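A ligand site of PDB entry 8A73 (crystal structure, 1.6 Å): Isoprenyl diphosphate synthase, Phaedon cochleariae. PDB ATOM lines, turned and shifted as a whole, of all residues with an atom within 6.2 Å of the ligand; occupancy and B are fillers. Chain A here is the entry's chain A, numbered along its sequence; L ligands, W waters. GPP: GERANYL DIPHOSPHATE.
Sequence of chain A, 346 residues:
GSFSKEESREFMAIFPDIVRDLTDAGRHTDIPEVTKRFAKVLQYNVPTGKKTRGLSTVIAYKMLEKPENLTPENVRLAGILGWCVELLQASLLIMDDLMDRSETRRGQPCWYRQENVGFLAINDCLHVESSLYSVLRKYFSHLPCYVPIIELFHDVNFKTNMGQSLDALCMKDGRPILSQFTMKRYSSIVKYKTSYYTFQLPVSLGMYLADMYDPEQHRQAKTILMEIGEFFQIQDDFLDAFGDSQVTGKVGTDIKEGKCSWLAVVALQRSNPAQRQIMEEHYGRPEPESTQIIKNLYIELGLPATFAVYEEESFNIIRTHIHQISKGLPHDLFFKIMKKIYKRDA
O1B of the ligand is in hydrogen-bond range of NE2 of Gln 89. OG1 of Thr 52 lies within hydrogen-bond range of O2A of the ligand, 2.8 Å away. N of Lys 51 is in hydrogen-bond range of O2B of the ligand. An oxygen (O2B) of the ligand sits at hydrogen-bond distance from the backbone NH (N) of Thr 52, at 2.9 Å. The guanidinium group of Arg 106 lies within salt-bridge range of an oxygen (O1B) of the ligand (2.7 Å). The guanidinium group (NH1) of Arg 53 lies within salt-bridge range of an oxygen (O1B) of the ligand (3.5 Å). The backbone NH of Lys 50 sits at hydrogen-bond distance from an oxygen (O3B) of the ligand (3.0 Å).
NH1 of Arg 53 sits close to OE1 of Gln 89, 3.1 Å away. The backbone carbonyl oxygen (O) of Thr 52 is in hydrogen-bond range of the side-chain hydroxyl (OG) of Ser 56 (2.7 Å). OG1 of Thr 57 sits at hydrogen-bond distance from O of Arg 53. NE of Arg 53 lies within hydrogen-bond range of OG1 of Thr 198 (3.0 Å). The backbone carbonyl oxygen (O) of Gly 49 lies within hydrogen-bond range of the side-chain amino group (NZ) of Lys 51 (2.8 Å). The side-chain carboxylate (OE1) of Glu 86 sits at hydrogen-bond distance from the side-chain amide nitrogen (NE2) of Gln 89, at 3.3 Å.
Residues that only touch the ligand: Ser 56 (3.4 Å), Thr 198 (3.4 Å), Phe 232 (3.7 Å), Ile 337 (3.7 Å), Ile 341 (3.8 Å), Gly 49 (3.8 Å), Phe 199 (3.9 Å) and Pro 202 (3.96 Å). Hydrophobic or aromatic side chains that line the ligand: Phe 199, Pro 202, Phe 232, Ile 337 and Ile 341. Of the 24 residues printed, 14 come within 4 Å of the ligand. Along chain A the residues within 4 Å of the ligand span positions 49 to 341. The nearest printed residue that does not touch the ligand is Arg 344 (4.1 Å).
Water W3 bridges an oxygen (O1A) of the ligand (2.7 Å) and the guanidinium group (NH2) of Arg 53 (2.9 Å). Water W4 lies within hydrogen-bond range of the side-chain carboxylate (OE1) of Glu 86, an oxygen (O1B) of the ligand, the backbone NH (N) of Lys 51 and the guanidinium group (NH2) of Arg 106. Water W1 lies within hydrogen-bond range of OE1 of Gln 89 (2.9 Å), O1B of the ligand (3.0 Å) and NH2 of Arg 106 (3.4 Å).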
ATOM      1  N   GLY A  49      34.070 -14.326 -35.833  1.00  0.00           N
ATOM      2  CA  GLY A  49      33.808 -14.551 -34.390  1.00  0.00           C
ATOM      3  C   GLY A  49      32.603 -15.460 -34.154  1.00  0.00           C
ATOM      4  O   GLY A  49      32.220 -16.207 -35.086  1.00  0.00           O
ATOM      5  N   LYS A  50      32.037 -15.409 -32.946  1.00  0.00           N
ATOM      6  CA  LYS A  50      30.792 -16.125 -32.567  1.00  0.00           C
ATOM      7  C   LYS A  50      29.571 -15.295 -32.978  1.00  0.00           C
ATOM      8  O   LYS A  50      28.459 -15.849 -33.018  1.00  0.00           O
ATOM      9  CB  LYS A  50      30.785 -16.399 -31.061  1.00  0.00           C
ATOM     10  CG  LYS A  50      31.953 -17.217 -30.546  1.00  0.00           C
ATOM     11  CD  LYS A  50      31.795 -17.682 -29.116  1.00  0.00           C
ATOM     12  CE  LYS A  50      30.957 -18.942 -28.988  1.00  0.00           C
ATOM     13  NZ  LYS A  50      30.650 -19.248 -27.580  1.00  0.00           N
ATOM     14  N   LYS A  51      29.772 -14.000 -33.257  1.00  0.00           N
ATOM     15  CA  LYS A  51      28.708 -13.007 -33.570  1.00  0.00           C
ATOM     16  C   LYS A  51      27.615 -13.081 -32.498  1.00  0.00           C
ATOM     17  O   LYS A  51      26.420 -13.020 -32.852  1.00  0.00           O
ATOM     18  CB  LYS A  51      28.120 -13.254 -34.971  1.00  0.00           C
ATOM     19  CG  LYS A  51      29.021 -12.862 -36.134  1.00  0.00           C
ATOM     20  CD  LYS A  51      30.096 -13.866 -36.465  1.00  0.00           C
ATOM     21  CE  LYS A  51      29.559 -15.243 -36.791  1.00  0.00           C
ATOM     22  NZ  LYS A  51      30.606 -16.092 -37.389  1.00  0.00           N
ATOM     23  N   THR A  52      27.988 -13.197 -31.218  1.00  0.00           N
ATOM     24  CA  THR A  52      27.021 -13.339 -30.098  1.00  0.00           C
ATOM     25  C   THR A  52      26.140 -12.100 -30.030  1.00  0.00           C
ATOM     26  O   THR A  52      24.907 -12.249 -29.841  1.00  0.00           O
ATOM     27  CB  THR A  52      27.731 -13.634 -28.773  1.00  0.00           C
ATOM     28  OG1 THR A  52      28.547 -14.786 -28.963  1.00  0.00           O
ATOM     29  CG2 THR A  52      26.753 -13.886 -27.643  1.00  0.00           C
ATOM     30  N   ARG A  53      26.709 -10.901 -30.191  1.00  0.00           N
ATOM     31  CA  ARG A  53      25.937  -9.631 -30.109  1.00  0.00           C
ATOM     32  C   ARG A  53      24.969  -9.545 -31.302  1.00  0.00           C
ATOM     33  O   ARG A  53      23.799  -9.163 -31.073  1.00  0.00           O
ATOM     34  CB  ARG A  53      26.882  -8.428 -30.051  1.00  0.00           C
ATOM     35  CG  ARG A  53      27.644  -8.313 -28.747  1.00  0.00           C
ATOM     36  CD  ARG A  53      28.868  -7.423 -28.890  1.00  0.00           C
ATOM     37  NE  ARG A  53      29.727  -7.470 -27.712  1.00  0.00           N
ATOM     38  CZ  ARG A  53      30.537  -8.483 -27.390  1.00  0.00           C
ATOM     39  NH1 ARG A  53      30.629  -9.556 -28.156  1.00  0.00           N
ATOM     40  NH2 ARG A  53      31.265  -8.402 -26.291  1.00  0.00           N
ATOM     41  N   SER A  56      22.204 -12.134 -30.870  1.00  0.00           N
ATOM     42  CA  SER A  56      21.398 -11.714 -29.689  1.00  0.00           C
ATOM     43  C   SER A  56      20.395 -10.614 -30.087  1.00  0.00           C
ATOM     44  O   SER A  56      19.318 -10.555 -29.468  1.00  0.00           O
ATOM     45  CB  SER A  56      22.268 -11.292 -28.538  1.00  0.00           C
ATOM     46  OG  SER A  56      22.916 -12.410 -27.962  1.00  0.00           O
ATOM     47  N   THR A  57      20.729  -9.790 -31.087  1.00  0.00           N
ATOM     48  CA  THR A  57      19.819  -8.762 -31.654  1.00  0.00           C
ATOM     49  C   THR A  57      18.597  -9.476 -32.250  1.00  0.00           C
ATOM     50  O   THR A  57      17.459  -9.053 -31.958  1.00  0.00           O
ATOM     51  CB  THR A  57      20.540  -7.879 -32.687  1.00  0.00           C
ATOM     52  OG1 THR A  57      21.720  -7.375 -32.073  1.00  0.00           O
ATOM     53  CG2 THR A  57      19.691  -6.730 -33.188  1.00  0.00           C
ATOM     54  N   ALA A  60      16.514 -11.119 -29.349  1.00  0.00           N
ATOM     55  CA  ALA A  60      15.817 -10.018 -28.660  1.00  0.00           C
ATOM     56  C   ALA A  60      14.565  -9.645 -29.450  1.00  0.00           C
ATOM     57  O   ALA A  60      13.471  -9.627 -28.853  1.00  0.00           O
ATOM     58  CB  ALA A  60      16.727  -8.833 -28.485  1.00  0.00           C
ATOM     59  N   GLU A  86      27.803  -5.877 -35.191  1.00  0.00           N
ATOM     60  CA  GLU A  86      29.098  -6.559 -35.449  1.00  0.00           C
ATOM     61  C   GLU A  86      30.027  -5.620 -36.214  1.00  0.00           C
ATOM     62  O   GLU A  86      31.244  -5.673 -35.949  1.00  0.00           O
ATOM     63  CB  GLU A  86      28.864  -7.893 -36.181  1.00  0.00           C
ATOM     64  CG  GLU A  86      28.156  -8.929 -35.325  1.00  0.00           C
ATOM     65  CD  GLU A  86      28.934  -9.456 -34.128  1.00  0.00           C
ATOM     66  OE1 GLU A  86      30.188  -9.464 -34.161  1.00  0.00           O
ATOM     67  OE2 GLU A  86      28.277  -9.870 -33.146  1.00  0.00           O
ATOM     68  N   GLN A  89      31.307  -3.229 -33.504  1.00  0.00           N
ATOM     69  CA  GLN A  89      32.280  -3.952 -32.642  1.00  0.00           C
ATOM     70  C   GLN A  89      33.623  -4.102 -33.377  1.00  0.00           C
ATOM     71  O   GLN A  89      34.672  -3.808 -32.755  1.00  0.00           O
ATOM     72  CB  GLN A  89      31.770  -5.326 -32.229  1.00  0.00           C
ATOM     73  CG  GLN A  89      32.807  -6.059 -31.399  1.00  0.00           C
ATOM     74  CD  GLN A  89      32.273  -7.288 -30.719  1.00  0.00           C
ATOM     75  OE1 GLN A  89      32.384  -7.436 -29.513  1.00  0.00           O
ATOM     76  NE2 GLN A  89      31.682  -8.174 -31.515  1.00  0.00           N
ATOM     77  N   LEU A  93      37.249  -2.818 -31.963  1.00  0.00           N
ATOM     78  CA  LEU A  93      38.328  -3.780 -31.618  1.00  0.00           C
ATOM     79  C   LEU A  93      39.532  -3.564 -32.538  1.00  0.00           C
ATOM     80  O   LEU A  93      40.658  -3.722 -32.030  1.00  0.00           O
ATOM     81  CB  LEU A  93      37.778  -5.212 -31.682  1.00  0.00           C
ATOM     82  CG  LEU A  93      36.603  -5.479 -30.748  1.00  0.00           C
ATOM     83  CD1 LEU A  93      36.226  -6.939 -30.740  1.00  0.00           C
ATOM     84  CD2 LEU A  93      36.895  -5.003 -29.328  1.00  0.00           C
ATOM     85  N   ARG A 106      40.597 -13.220 -31.287  1.00  0.00           N
ATOM     86  CA  ARG A 106      39.888 -14.470 -31.697  1.00  0.00           C
ATOM     87  C   ARG A 106      40.829 -15.382 -32.490  1.00  0.00           C
ATOM     88  O   ARG A 106      40.376 -15.941 -33.515  1.00  0.00           O
ATOM     89  CB  ARG A 106      38.639 -14.137 -32.516  1.00  0.00           C
ATOM     90  CG  ARG A 106      37.628 -13.266 -31.802  1.00  0.00           C
ATOM     91  CD  ARG A 106      36.256 -13.370 -32.428  1.00  0.00           C
ATOM     92  NE  ARG A 106      35.395 -12.275 -32.032  1.00  0.00           N
ATOM     93  CZ  ARG A 106      35.451 -11.033 -32.520  1.00  0.00           C
ATOM     94  NH1 ARG A 106      36.361 -10.718 -33.429  1.00  0.00           N
ATOM     95  NH2 ARG A 106      34.615 -10.117 -32.077  1.00  0.00           N
ATOM     96  N   THR A 198      27.334  -3.884 -25.970  1.00  0.00           N
ATOM     97  CA  THR A 198      27.257  -5.363 -25.873  1.00  0.00           C
ATOM     98  C   THR A 198      25.823  -5.789 -25.513  1.00  0.00           C
ATOM     99  O   THR A 198      25.325  -6.712 -26.165  1.00  0.00           O
ATOM    100  CB  THR A 198      28.274  -5.933 -24.888  1.00  0.00           C
ATOM    101  OG1 THR A 198      29.585  -5.619 -25.383  1.00  0.00           O
ATOM    102  CG2 THR A 198      28.136  -7.420 -24.698  1.00  0.00           C
ATOM    103  N   PHE A 199      25.202  -5.133 -24.534  1.00  0.00           N
ATOM    104  CA  PHE A 199      23.899  -5.546 -23.936  1.00  0.00           C
ATOM    105  C   PHE A 199      22.773  -4.585 -24.317  1.00  0.00           C
ATOM    106  O   PHE A 199      21.752  -5.066 -24.831  1.00  0.00           O
ATOM    107  CB  PHE A 199      24.051  -5.708 -22.422  1.00  0.00           C
ATOM    108  CG  PHE A 199      24.855  -6.920 -22.047  1.00  0.00           C
ATOM    109  CD1 PHE A 199      24.280  -8.182 -22.077  1.00  0.00           C
ATOM    110  CD2 PHE A 199      26.190  -6.811 -21.688  1.00  0.00           C
ATOM    111  CE1 PHE A 199      25.021  -9.305 -21.762  1.00  0.00           C
ATOM    112  CE2 PHE A 199      26.929  -7.933 -21.353  1.00  0.00           C
ATOM    113  CZ  PHE A 199      26.345  -9.186 -21.395  1.00  0.00           C
ATOM    114  N   GLN A 200      22.930  -3.280 -24.088  1.00  0.00           N
ATOM    115  CA  GLN A 200      21.837  -2.297 -24.324  1.00  0.00           C
ATOM    116  C   GLN A 200      21.532  -2.244 -25.825  1.00  0.00           C
ATOM    117  O   GLN A 200      20.348  -2.263 -26.187  1.00  0.00           O
ATOM    118  CB  GLN A 200      22.187  -0.906 -23.800  1.00  0.00           C
ATOM    119  CG  GLN A 200      20.975   0.013 -23.728  1.00  0.00           C
ATOM    120  CD  GLN A 200      21.286   1.469 -24.006  1.00  0.00           C
ATOM    121  OE1 GLN A 200      21.961   1.803 -24.975  1.00  0.00           O
ATOM    122  NE2 GLN A 200      20.770   2.343 -23.149  1.00  0.00           N
ATOM    123  N   PRO A 202      21.911  -4.354 -28.664  1.00  0.00           N
ATOM    124  CA  PRO A 202      21.074  -5.407 -29.266  1.00  0.00           C
ATOM    125  C   PRO A 202      19.599  -5.382 -28.838  1.00  0.00           C
ATOM    126  O   PRO A 202      18.739  -5.539 -29.690  1.00  0.00           O
ATOM    127  CB  PRO A 202      21.767  -6.697 -28.803  1.00  0.00           C
ATOM    128  CG  PRO A 202      23.207  -6.281 -28.648  1.00  0.00           C
ATOM    129  CD  PRO A 202      23.124  -4.900 -28.037  1.00  0.00           C
ATOM    130  N   VAL A 203      19.333  -5.180 -27.544  1.00  0.00           N
ATOM    131  CA  VAL A 203      17.943  -5.193 -26.994  1.00  0.00           C
ATOM    132  C   VAL A 203      17.193  -3.953 -27.484  1.00  0.00           C
ATOM    133  O   VAL A 203      16.042  -4.104 -27.939  1.00  0.00           O
ATOM    134  CB  VAL A 203      17.932  -5.316 -25.461  1.00  0.00           C
ATOM    135  CG1 VAL A 203      16.529  -5.149 -24.895  1.00  0.00           C
ATOM    136  CG2 VAL A 203      18.526  -6.647 -25.010  1.00  0.00           C
ATOM    137  N   LEU A 225      20.040  -4.486 -17.849  1.00  0.00           N
ATOM    138  CA  LEU A 225      21.110  -4.870 -18.806  1.00  0.00           C
ATOM    139  C   LEU A 225      22.468  -4.359 -18.321  1.00  0.00           C
ATOM    140  O   LEU A 225      23.469  -5.051 -18.565  1.00  0.00           O
ATOM    141  CB  LEU A 225      20.761  -4.356 -20.210  1.00  0.00           C
ATOM    142  CG  LEU A 225      19.623  -5.101 -20.906  1.00  0.00           C
ATOM    143  CD1 LEU A 225      19.183  -4.374 -22.154  1.00  0.00           C
ATOM    144  CD2 LEU A 225      20.025  -6.536 -21.243  1.00  0.00           C
ATOM    145  N   PHE A 232      28.803  -9.949 -16.252  1.00  0.00           N
ATOM    146  CA  PHE A 232      29.459 -10.558 -17.429  1.00  0.00           C
ATOM    147  C   PHE A 232      30.944 -10.166 -17.470  1.00  0.00           C
ATOM    148  O   PHE A 232      31.781 -11.058 -17.681  1.00  0.00           O
ATOM    149  CB  PHE A 232      28.744 -10.153 -18.726  1.00  0.00           C
ATOM    150  CG  PHE A 232      29.325 -10.813 -19.951  1.00  0.00           C
ATOM    151  CD1 PHE A 232      29.157 -12.168 -20.171  1.00  0.00           C
ATOM    152  CD2 PHE A 232      30.081 -10.088 -20.856  1.00  0.00           C
ATOM    153  CE1 PHE A 232      29.705 -12.777 -21.290  1.00  0.00           C
ATOM    154  CE2 PHE A 232      30.629 -10.697 -21.976  1.00  0.00           C
ATOM    155  CZ  PHE A 232      30.440 -12.041 -22.188  1.00  0.00           C
ATOM    156  N   ILE A 337      18.923 -14.416 -21.023  1.00  0.00           N
ATOM    157  CA  ILE A 337      20.287 -13.803 -20.992  1.00  0.00           C
ATOM    158  C   ILE A 337      21.021 -14.349 -19.760  1.00  0.00           C
ATOM    159  O   ILE A 337      22.134 -14.870 -19.933  1.00  0.00           O
ATOM    160  CB  ILE A 337      20.223 -12.263 -21.017  1.00  0.00           C
ATOM    161  CG1 ILE A 337      19.620 -11.737 -22.322  1.00  0.00           C
ATOM    162  CG2 ILE A 337      21.599 -11.655 -20.763  1.00  0.00           C
ATOM    163  CD1 ILE A 337      19.226 -10.277 -22.287  1.00  0.00           C
ATOM    164  N   LYS A 340      22.052 -18.090 -19.887  1.00  0.00           N
ATOM    165  CA  LYS A 340      23.224 -18.253 -20.784  1.00  0.00           C
ATOM    166  C   LYS A 340      24.509 -17.897 -20.033  1.00  0.00           C
ATOM    167  O   LYS A 340      25.509 -18.627 -20.186  1.00  0.00           O
ATOM    168  CB  LYS A 340      23.053 -17.345 -22.012  1.00  0.00           C
ATOM    169  CG  LYS A 340      24.072 -17.543 -23.129  1.00  0.00           C
ATOM    170  CD  LYS A 340      24.339 -16.276 -23.934  1.00  0.00           C
ATOM    171  CE  LYS A 340      24.753 -16.551 -25.359  1.00  0.00           C
ATOM    172  NZ  LYS A 340      25.986 -17.360 -25.441  1.00  0.00           N
ATOM    173  N   ILE A 341      24.474 -16.823 -19.240  1.00  0.00           N
ATOM    174  CA  ILE A 341      25.665 -16.081 -18.719  1.00  0.00           C
ATOM    175  C   ILE A 341      26.212 -16.757 -17.439  1.00  0.00           C
ATOM    176  O   ILE A 341      27.441 -16.791 -17.272  1.00  0.00           O
ATOM    177  CB  ILE A 341      25.305 -14.597 -18.478  1.00  0.00           C
ATOM    178  CG1 ILE A 341      24.829 -13.911 -19.760  1.00  0.00           C
ATOM    179  CG2 ILE A 341      26.451 -13.843 -17.842  1.00  0.00           C
ATOM    180  CD1 ILE A 341      25.928 -13.404 -20.658  1.00  0.00           C
ATOM    181  N   ARG A 344      29.293 -19.729 -16.271  1.00  0.00           N
ATOM    182  CA  ARG A 344      30.065 -20.030 -17.509  1.00  0.00           C
ATOM    183  C   ARG A 344      31.566 -20.091 -17.177  1.00  0.00           C
ATOM    184  O   ARG A 344      32.003 -19.354 -16.277  1.00  0.00           O
ATOM    185  CB  ARG A 344      29.787 -19.000 -18.610  1.00  0.00           C
ATOM    186  CG  ARG A 344      28.925 -19.532 -19.748  1.00  0.00           C
ATOM    187  CD  ARG A 344      28.456 -18.450 -20.704  1.00  0.00           C
ATOM    188  NE  ARG A 344      29.517 -17.902 -21.537  1.00  0.00           N
ATOM    189  CZ  ARG A 344      29.339 -16.979 -22.473  1.00  0.00           C
ATOM    190  NH1 ARG A 344      28.124 -16.486 -22.686  1.00  0.00           N
ATOM    191  NH2 ARG A 344      30.363 -16.539 -23.178  1.00  0.00           N
ATOM    192  N   ALA A 346      33.787 -19.903 -19.843  1.00  0.00           N
ATOM    193  CA  ALA A 346      34.321 -19.263 -21.057  1.00  0.00           C
ATOM    194  C   ALA A 346      33.332 -18.214 -21.563  1.00  0.00           C
ATOM    195  O   ALA A 346      33.603 -17.511 -22.539  1.00  0.00           O
ATOM    196  CB  ALA A 346      34.600 -20.312 -22.112  1.00  0.00           C
ATOM    197  OXT ALA A 346      32.244 -18.037 -21.018  1.00  0.00           O
HETATM  198  C1  GPP L   1      29.751 -12.467 -25.816  1.00  0.00           C
HETATM  199  O1  GPP L   1      30.570 -12.236 -26.957  1.00  0.00           O
HETATM  200  C2  GPP L   1      28.623 -11.479 -25.775  1.00  0.00           C
HETATM  201  C3  GPP L   1      27.507 -11.599 -25.077  1.00  0.00           C
HETATM  202  C4  GPP L   1      27.224 -12.753 -24.155  1.00  0.00           C
HETATM  203  C5  GPP L   1      26.413 -10.572 -25.153  1.00  0.00           C
HETATM  204  C6  GPP L   1      25.259 -10.941 -26.059  1.00  0.00           C
HETATM  205  C7  GPP L   1      24.152  -9.923 -26.025  1.00  0.00           C
HETATM  206  C8  GPP L   1      22.977  -9.985 -25.416  1.00  0.00           C
HETATM  207  C9  GPP L   1      21.975  -8.878 -25.502  1.00  0.00           C
HETATM  208  C10 GPP L   1      22.535 -11.161 -24.595  1.00  0.00           C
HETATM  209  PA  GPP L   1      31.729 -13.270 -27.316  1.00  0.00           P
HETATM  210  O1A GPP L   1      32.695 -13.297 -26.186  1.00  0.00           O
HETATM  211  O2A GPP L   1      31.095 -14.549 -27.757  1.00  0.00           O
HETATM  212  O3A GPP L   1      32.419 -12.550 -28.572  1.00  0.00           O
HETATM  213  PB  GPP L   1      32.147 -12.539 -30.170  1.00  0.00           P
HETATM  214  O1B GPP L   1      32.541 -11.156 -30.628  1.00  0.00           O
HETATM  215  O2B GPP L   1      30.691 -12.836 -30.369  1.00  0.00           O
HETATM  216  O3B GPP L   1      33.062 -13.618 -30.751  1.00  0.00           O
HETATM  217  O   HOH W   1      34.191  -9.589 -28.743  1.00  0.00           O
HETATM  218  O   HOH W   2      29.529 -10.276 -30.833  1.00  0.00           O
HETATM  219  O   HOH W   3      32.811 -10.675 -25.521  1.00  0.00           O
HETATM  220  O   HOH W   4      31.682 -11.455 -33.231  1.00  0.00           O
